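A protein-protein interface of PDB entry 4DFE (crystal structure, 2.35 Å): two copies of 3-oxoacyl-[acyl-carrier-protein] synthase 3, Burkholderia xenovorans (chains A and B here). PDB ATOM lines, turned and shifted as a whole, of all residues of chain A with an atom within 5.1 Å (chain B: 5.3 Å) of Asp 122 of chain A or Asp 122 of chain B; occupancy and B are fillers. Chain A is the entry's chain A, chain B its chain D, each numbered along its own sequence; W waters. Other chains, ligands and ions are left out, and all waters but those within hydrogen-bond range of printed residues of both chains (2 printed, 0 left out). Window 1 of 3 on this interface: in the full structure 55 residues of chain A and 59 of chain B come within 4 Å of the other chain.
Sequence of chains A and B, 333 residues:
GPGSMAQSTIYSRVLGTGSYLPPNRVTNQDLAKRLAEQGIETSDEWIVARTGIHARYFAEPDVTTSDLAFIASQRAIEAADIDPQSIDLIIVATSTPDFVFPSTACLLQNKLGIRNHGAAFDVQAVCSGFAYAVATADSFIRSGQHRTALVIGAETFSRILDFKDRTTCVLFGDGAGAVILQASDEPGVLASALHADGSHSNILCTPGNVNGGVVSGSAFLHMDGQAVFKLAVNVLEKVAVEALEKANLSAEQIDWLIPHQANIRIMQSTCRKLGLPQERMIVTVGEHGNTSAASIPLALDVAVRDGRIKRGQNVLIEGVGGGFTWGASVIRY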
ATOM      1  N   VAL A  92     -30.650 -20.904 -20.044  1.00  0.00           N
ATOM      2  CA  VAL A  92     -29.995 -20.362 -21.263  1.00  0.00           C
ATOM      3  C   VAL A  92     -28.739 -21.154 -21.666  1.00  0.00           C
ATOM      4  O   VAL A  92     -27.801 -21.285 -20.885  1.00  0.00           O
ATOM      5  CB  VAL A  92     -29.581 -18.900 -21.058  1.00  0.00           C
ATOM      6  CG1 VAL A  92     -28.689 -18.420 -22.188  1.00  0.00           C
ATOM      7  CG2 VAL A  92     -30.821 -18.019 -20.882  1.00  0.00           C
ATOM      8  N   THR A  94     -25.644 -20.814 -23.847  1.00  0.00           N
ATOM      9  CA  THR A  94     -24.797 -19.845 -24.534  1.00  0.00           C
ATOM     10  C   THR A  94     -23.322 -20.080 -24.213  1.00  0.00           C
ATOM     11  O   THR A  94     -22.975 -20.622 -23.180  1.00  0.00           O
ATOM     12  CB  THR A  94     -25.134 -18.402 -24.138  1.00  0.00           C
ATOM     13  OG1 THR A  94     -24.450 -17.472 -24.999  1.00  0.00           O
ATOM     14  CG2 THR A  94     -24.723 -18.156 -22.709  1.00  0.00           C
ATOM     15  N   PRO A  97     -21.984 -15.366 -22.873  1.00  0.00           N
ATOM     16  CA  PRO A  97     -22.817 -14.679 -21.907  1.00  0.00           C
ATOM     17  C   PRO A  97     -22.412 -13.206 -21.765  1.00  0.00           C
ATOM     18  O   PRO A  97     -21.239 -12.867 -22.004  1.00  0.00           O
ATOM     19  CB  PRO A  97     -22.547 -15.439 -20.604  1.00  0.00           C
ATOM     20  CG  PRO A  97     -21.168 -15.973 -20.770  1.00  0.00           C
ATOM     21  CD  PRO A  97     -21.014 -16.275 -22.232  1.00  0.00           C
ATOM     22  N   SER A 103     -25.138 -14.940 -14.488  1.00  0.00           N
ATOM     23  CA  SER A 103     -25.623 -15.645 -15.676  1.00  0.00           C
ATOM     24  C   SER A 103     -26.549 -14.818 -16.531  1.00  0.00           C
ATOM     25  O   SER A 103     -27.282 -13.949 -16.045  1.00  0.00           O
ATOM     26  CB  SER A 103     -26.397 -16.903 -15.254  1.00  0.00           C
ATOM     27  OG  SER A 103     -27.613 -16.557 -14.600  1.00  0.00           O
ATOM     28  N   THR A 104     -26.523 -15.135 -17.824  1.00  0.00           N
ATOM     29  CA  THR A 104     -27.461 -14.594 -18.793  1.00  0.00           C
ATOM     30  C   THR A 104     -28.925 -14.874 -18.393  1.00  0.00           C
ATOM     31  O   THR A 104     -29.827 -14.069 -18.649  1.00  0.00           O
ATOM     32  CB  THR A 104     -27.189 -15.226 -20.167  1.00  0.00           C
ATOM     33  OG1 THR A 104     -25.761 -15.241 -20.421  1.00  0.00           O
ATOM     34  CG2 THR A 104     -27.948 -14.513 -21.239  1.00  0.00           C
ATOM     35  N   ALA A 105     -29.174 -16.042 -17.837  1.00  0.00           N
ATOM     36  CA  ALA A 105     -30.538 -16.384 -17.479  1.00  0.00           C
ATOM     37  C   ALA A 105     -31.064 -15.402 -16.439  1.00  0.00           C
ATOM     38  O   ALA A 105     -32.237 -15.010 -16.479  1.00  0.00           O
ATOM     39  CB  ALA A 105     -30.580 -17.779 -16.910  1.00  0.00           C
ATOM     40  N   ALA A 120     -32.854 -19.846 -12.270  1.00  0.00           N
ATOM     41  CA  ALA A 120     -32.336 -19.370 -13.551  1.00  0.00           C
ATOM     42  C   ALA A 120     -30.812 -19.642 -13.627  1.00  0.00           C
ATOM     43  O   ALA A 120     -30.041 -19.256 -12.720  1.00  0.00           O
ATOM     44  CB  ALA A 120     -32.619 -17.900 -13.718  1.00  0.00           C
ATOM     45  N   PHE A 121     -30.399 -20.349 -14.674  1.00  0.00           N
ATOM     46  CA  PHE A 121     -28.963 -20.630 -14.915  1.00  0.00           C
ATOM     47  C   PHE A 121     -28.589 -20.846 -16.385  1.00  0.00           C
ATOM     48  O   PHE A 121     -29.457 -21.070 -17.225  1.00  0.00           O
ATOM     49  CB  PHE A 121     -28.470 -21.809 -14.065  1.00  0.00           C
ATOM     50  CG  PHE A 121     -29.111 -23.147 -14.382  1.00  0.00           C
ATOM     51  CD1 PHE A 121     -28.387 -24.148 -15.022  1.00  0.00           C
ATOM     52  CD2 PHE A 121     -30.369 -23.448 -13.919  1.00  0.00           C
ATOM     53  CE1 PHE A 121     -28.944 -25.401 -15.245  1.00  0.00           C
ATOM     54  CE2 PHE A 121     -30.919 -24.696 -14.118  1.00  0.00           C
ATOM     55  CZ  PHE A 121     -30.206 -25.679 -14.798  1.00  0.00           C
ATOM     56  N   ASP A 122     -27.295 -20.751 -16.662  1.00  0.00           N
ATOM     57  CA  ASP A 122     -26.753 -21.039 -17.964  1.00  0.00           C
ATOM     58  C   ASP A 122     -26.076 -22.426 -17.960  1.00  0.00           C
ATOM     59  O   ASP A 122     -25.518 -22.864 -16.936  1.00  0.00           O
ATOM     60  CB  ASP A 122     -25.702 -19.992 -18.355  1.00  0.00           C
ATOM     61  CG  ASP A 122     -26.270 -18.589 -18.501  1.00  0.00           C
ATOM     62  OD1 ASP A 122     -27.503 -18.371 -18.371  1.00  0.00           O
ATOM     63  OD2 ASP A 122     -25.468 -17.648 -18.775  1.00  0.00           O
ATOM     64  N   VAL A 123     -26.106 -23.081 -19.121  1.00  0.00           N
ATOM     65  CA  VAL A 123     -25.362 -24.297 -19.363  1.00  0.00           C
ATOM     66  C   VAL A 123     -24.416 -24.084 -20.552  1.00  0.00           C
ATOM     67  O   VAL A 123     -24.738 -23.335 -21.501  1.00  0.00           O
ATOM     68  CB  VAL A 123     -26.298 -25.474 -19.656  1.00  0.00           C
ATOM     69  CG1 VAL A 123     -27.142 -25.814 -18.440  1.00  0.00           C
ATOM     70  CG2 VAL A 123     -27.168 -25.163 -20.856  1.00  0.00           C
ATOM     71  N   GLN A 124     -23.240 -24.728 -20.489  1.00  0.00           N
ATOM     72  CA  GLN A 124     -22.222 -24.652 -21.537  1.00  0.00           C
ATOM     73  C   GLN A 124     -21.945 -26.032 -22.232  1.00  0.00           C
ATOM     74  O   GLN A 124     -21.307 -26.920 -21.663  1.00  0.00           O
ATOM     75  CB  GLN A 124     -20.928 -24.102 -20.938  1.00  0.00           C
ATOM     76  CG  GLN A 124     -19.713 -24.183 -21.864  1.00  0.00           C
ATOM     77  CD  GLN A 124     -19.834 -23.314 -23.103  1.00  0.00           C
ATOM     78  OE1 GLN A 124     -20.812 -23.401 -23.852  1.00  0.00           O
ATOM     79  NE2 GLN A 124     -18.818 -22.513 -23.353  1.00  0.00           N
ATOM     80  N   VAL B  92     -19.642 -29.649 -14.055  1.00  0.00           N
ATOM     81  CA  VAL B  92     -18.821 -28.700 -13.346  1.00  0.00           C
ATOM     82  C   VAL B  92     -19.572 -27.332 -13.107  1.00  0.00           C
ATOM     83  O   VAL B  92     -19.966 -26.654 -14.042  1.00  0.00           O
ATOM     84  CB  VAL B  92     -17.530 -28.437 -14.123  1.00  0.00           C
ATOM     85  CG1 VAL B  92     -16.712 -27.330 -13.458  1.00  0.00           C
ATOM     86  CG2 VAL B  92     -16.701 -29.704 -14.237  1.00  0.00           C
ATOM     87  N   THR B  94     -18.755 -23.728 -12.250  1.00  0.00           N
ATOM     88  CA  THR B  94     -17.687 -22.734 -12.184  1.00  0.00           C
ATOM     89  C   THR B  94     -18.112 -21.427 -12.867  1.00  0.00           C
ATOM     90  O   THR B  94     -19.009 -21.398 -13.684  1.00  0.00           O
ATOM     91  CB  THR B  94     -16.442 -23.218 -12.878  1.00  0.00           C
ATOM     92  OG1 THR B  94     -15.348 -22.318 -12.613  1.00  0.00           O
ATOM     93  CG2 THR B  94     -16.743 -23.307 -14.370  1.00  0.00           C
ATOM     94  N   PRO B  97     -14.238 -20.758 -15.912  1.00  0.00           N
ATOM     95  CA  PRO B  97     -13.773 -21.861 -16.757  1.00  0.00           C
ATOM     96  C   PRO B  97     -12.423 -21.554 -17.449  1.00  0.00           C
ATOM     97  O   PRO B  97     -12.117 -20.385 -17.711  1.00  0.00           O
ATOM     98  CB  PRO B  97     -14.890 -22.007 -17.771  1.00  0.00           C
ATOM     99  CG  PRO B  97     -15.503 -20.646 -17.874  1.00  0.00           C
ATOM    100  CD  PRO B  97     -15.351 -20.010 -16.527  1.00  0.00           C
ATOM    101  N   SER B 103     -16.179 -26.379 -22.624  1.00  0.00           N
ATOM    102  CA  SER B 103     -16.448 -26.452 -21.193  1.00  0.00           C
ATOM    103  C   SER B 103     -15.313 -27.074 -20.391  1.00  0.00           C
ATOM    104  O   SER B 103     -14.583 -27.945 -20.883  1.00  0.00           O
ATOM    105  CB  SER B 103     -17.709 -27.282 -20.945  1.00  0.00           C
ATOM    106  OG  SER B 103     -17.492 -28.636 -21.259  1.00  0.00           O
ATOM    107  N   THR B 104     -15.216 -26.646 -19.144  1.00  0.00           N
ATOM    108  CA  THR B 104     -14.337 -27.243 -18.162  1.00  0.00           C
ATOM    109  C   THR B 104     -14.623 -28.746 -17.979  1.00  0.00           C
ATOM    110  O   THR B 104     -13.724 -29.532 -17.717  1.00  0.00           O
ATOM    111  CB  THR B 104     -14.543 -26.526 -16.802  1.00  0.00           C
ATOM    112  OG1 THR B 104     -14.547 -25.105 -17.011  1.00  0.00           O
ATOM    113  CG2 THR B 104     -13.507 -26.904 -15.812  1.00  0.00           C
ATOM    114  N   ALA B 105     -15.895 -29.131 -18.057  1.00  0.00           N
ATOM    115  CA  ALA B 105     -16.265 -30.521 -17.812  1.00  0.00           C
ATOM    116  C   ALA B 105     -15.633 -31.385 -18.899  1.00  0.00           C
ATOM    117  O   ALA B 105     -15.114 -32.477 -18.625  1.00  0.00           O
ATOM    118  CB  ALA B 105     -17.785 -30.689 -17.763  1.00  0.00           C
ATOM    119  N   CYS B 106     -15.603 -30.855 -20.135  1.00  0.00           N
ATOM    120  CA  CYS B 106     -15.000 -31.577 -21.267  1.00  0.00           C
ATOM    121  C   CYS B 106     -13.508 -31.750 -21.089  1.00  0.00           C
ATOM    122  O   CYS B 106     -12.964 -32.820 -21.395  1.00  0.00           O
ATOM    123  CB  CYS B 106     -15.275 -30.857 -22.576  1.00  0.00           C
ATOM    124  SG  CYS B 106     -16.915 -31.136 -23.250  1.00  0.00           S
ATOM    125  N   ALA B 120     -20.884 -34.241 -20.702  1.00  0.00           N
ATOM    126  CA  ALA B 120     -20.124 -33.340 -19.863  1.00  0.00           C
ATOM    127  C   ALA B 120     -20.533 -31.877 -20.171  1.00  0.00           C
ATOM    128  O   ALA B 120     -20.471 -31.431 -21.345  1.00  0.00           O
ATOM    129  CB  ALA B 120     -18.647 -33.560 -20.086  1.00  0.00           C
ATOM    130  N   PHE B 121     -20.923 -31.135 -19.133  1.00  0.00           N
ATOM    131  CA  PHE B 121     -21.198 -29.685 -19.251  1.00  0.00           C
ATOM    132  C   PHE B 121     -20.988 -28.851 -17.970  1.00  0.00           C
ATOM    133  O   PHE B 121     -20.829 -29.384 -16.876  1.00  0.00           O
ATOM    134  CB  PHE B 121     -22.576 -29.446 -19.810  1.00  0.00           C
ATOM    135  CG  PHE B 121     -23.698 -29.905 -18.929  1.00  0.00           C
ATOM    136  CD1 PHE B 121     -24.494 -28.971 -18.236  1.00  0.00           C
ATOM    137  CD2 PHE B 121     -24.037 -31.235 -18.854  1.00  0.00           C
ATOM    138  CE1 PHE B 121     -25.581 -29.402 -17.494  1.00  0.00           C
ATOM    139  CE2 PHE B 121     -25.137 -31.651 -18.110  1.00  0.00           C
ATOM    140  CZ  PHE B 121     -25.899 -30.747 -17.424  1.00  0.00           C
ATOM    141  N   ASP B 122     -20.906 -27.537 -18.155  1.00  0.00           N
ATOM    142  CA  ASP B 122     -20.782 -26.587 -17.054  1.00  0.00           C
ATOM    143  C   ASP B 122     -22.111 -25.904 -16.837  1.00  0.00           C
ATOM    144  O   ASP B 122     -22.890 -25.675 -17.794  1.00  0.00           O
ATOM    145  CB  ASP B 122     -19.735 -25.506 -17.371  1.00  0.00           C
ATOM    146  CG  ASP B 122     -18.286 -26.069 -17.551  1.00  0.00           C
ATOM    147  OD1 ASP B 122     -18.041 -27.284 -17.334  1.00  0.00           O
ATOM    148  OD2 ASP B 122     -17.368 -25.250 -17.846  1.00  0.00           O
ATOM    149  N   VAL B 123     -22.374 -25.564 -15.582  1.00  0.00           N
ATOM    150  CA  VAL B 123     -23.519 -24.754 -15.199  1.00  0.00           C
ATOM    151  C   VAL B 123     -23.028 -23.507 -14.482  1.00  0.00           C
ATOM    152  O   VAL B 123     -21.976 -23.524 -13.806  1.00  0.00           O
ATOM    153  CB  VAL B 123     -24.440 -25.550 -14.259  1.00  0.00           C
ATOM    154  CG1 VAL B 123     -24.878 -26.895 -14.938  1.00  0.00           C
ATOM    155  CG2 VAL B 123     -23.719 -25.895 -12.937  1.00  0.00           C
ATOM    156  N   GLN B 124     -23.760 -22.411 -14.654  1.00  0.00           N
ATOM    157  CA  GLN B 124     -23.413 -21.124 -14.063  1.00  0.00           C
ATOM    158  C   GLN B 124     -24.496 -20.673 -13.090  1.00  0.00           C
ATOM    159  O   GLN B 124     -25.589 -20.189 -13.491  1.00  0.00           O
ATOM    160  CB  GLN B 124     -23.223 -20.077 -15.180  1.00  0.00           C
ATOM    161  CG  GLN B 124     -23.107 -18.632 -14.722  1.00  0.00           C
ATOM    162  CD  GLN B 124     -21.831 -18.380 -13.942  1.00  0.00           C
ATOM    163  OE1 GLN B 124     -21.603 -18.997 -12.882  1.00  0.00           O
ATOM    164  NE2 GLN B 124     -20.971 -17.471 -14.455  1.00  0.00           N
HETATM  165  O   HOH W   1     -19.878 -29.080 -22.389  1.00  0.00           O
HETATM  166  O   HOH W   2     -27.610 -18.309 -12.650  1.00  0.00           O
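The backbone carbonyl oxygen of Asp 122 of chain B sits at hydrogen-bond distance from the backbone NH of Gln 124 of chain A, at 2.9 Å. O of Asp 122 of chain A lies within hydrogen-bond range of N of Gln 124 of chain B, 2.9 Å away.
The backbone carbonyl oxygen (O) of Phe 121 of chain B lies within hydrogen-bond range of the backbone NH (N) of Val 92 of chain B (3.1 Å). N of Ala 105 of chain B sits at hydrogen-bond distance from OD1 of Asp 122 of chain B. OD2 of Asp 122 of chain A lies within hydrogen-bond range of N of Thr 104 of chain A (2.9 Å). N of Thr 104 of chain B lies within hydrogen-bond range of OD2 of Asp 122 of chain B, at 2.9 Å. The backbone NH (N) of Ala 105 of chain A sits at hydrogen-bond distance from the side-chain carboxylate (OD1) of Asp 122 of chain A. The backbone carbonyl oxygen (O) of Phe 121 of chain A lies within hydrogen-bond range of the backbone NH (N) of Val 92 of chain A, 3.1 Å away.
Gln 124 of chain B touches Ser 103 of chain A (CG to CB, 3.8 Å). CB of Phe 121 of chain A touches O of Gln 124 of chain B, 3.4 Å away. O of Asp 122 of chain A touches O of Asp 122 of chain B (3.9 Å). O of Asp 122 of chain A touches CA of Val 123 of chain B (3.3 Å). CA of Val 123 of chain A touches O of Asp 122 of chain B (3.2 Å). O of Gln 124 of chain A touches CB of Ser 103 of chain B, 3.7 Å away. CB of Phe 121 of chain B touches O of Gln 124 of chain A, 3.4 Å away.
Of the printed residues of chain B, Phe 121 of chain A touches Gln 124 (3.4 Å). Asp 122 of chain A touches just these residues of chain B: Asp 122, Val 123 and Gln 124. Printed residues of chain A within 4 Å of Phe 121 of chain B: Gln 124 (3.4 Å). Asp 122 of chain B touches three residues of chain A. Of the printed residues of chain A, Gln 124 of chain B touches Ser 103, Phe 121 and Asp 122. The nearest printed residue of chain B that does not touch Asp 122 of chain A is Phe 121 of chain B (6.3 Å). The nearest printed residue of chain A that does not touch Asp 122 of chain B is Phe 121 of chain A (6.3 Å).
Of the 12 printed residues of chain B, 5 touch a printed residue of chain A. Printed residues of chain A that touch a printed residue of chain B: Ser 103, Phe 121, Asp 122, Val 123 and Gln 124. Hydrophobic or aromatic side chains of chain A within 4 Å of the printed part of chain B: Phe 121 and Val 123. Among the printed residues, no Asp or Glu carboxylate lies within 4 Å of a Lys or Arg side-chain nitrogen of the other chain.
Ser 103 of chain A touches Gln 124 of chain B, and with the chains exchanged Gln 124 of chain A touches Ser 103 of chain B. Phe 121 of chain A touches Gln 124 of chain B, and with the chains exchanged Gln 124 of chain A touches Phe 121 of chain B. Asp 122 of chain A touches Val 123 of chain B, and with the chains exchanged Val 123 of chain A touches Asp 122 of chain B. Asp 122 of chain A touches Gln 124 of chain B, and with the chains exchanged Gln 124 of chain A touches Asp 122 of chain B. Positions printed for both chains: 92, 94, 97, 103, 104, 105, 120, 121, 122, 123 and 124. Of the 9 pairs that touch across the chains among the printed residues, 9 have their exchanged pair printed and touching as well.
Water W2 lies within hydrogen-bond range of the backbone carbonyl oxygen of Ala 120 of chain A, the side-chain hydroxyl of Ser 103 of chain A and the backbone carbonyl oxygen of Gln 124 of chain B. Water W1 lies within hydrogen-bond range of O of Ala 120 of chain B, OG of Ser 103 of chain B, O of Gln 124 of chain A and SG of Cys 106 of chain B.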
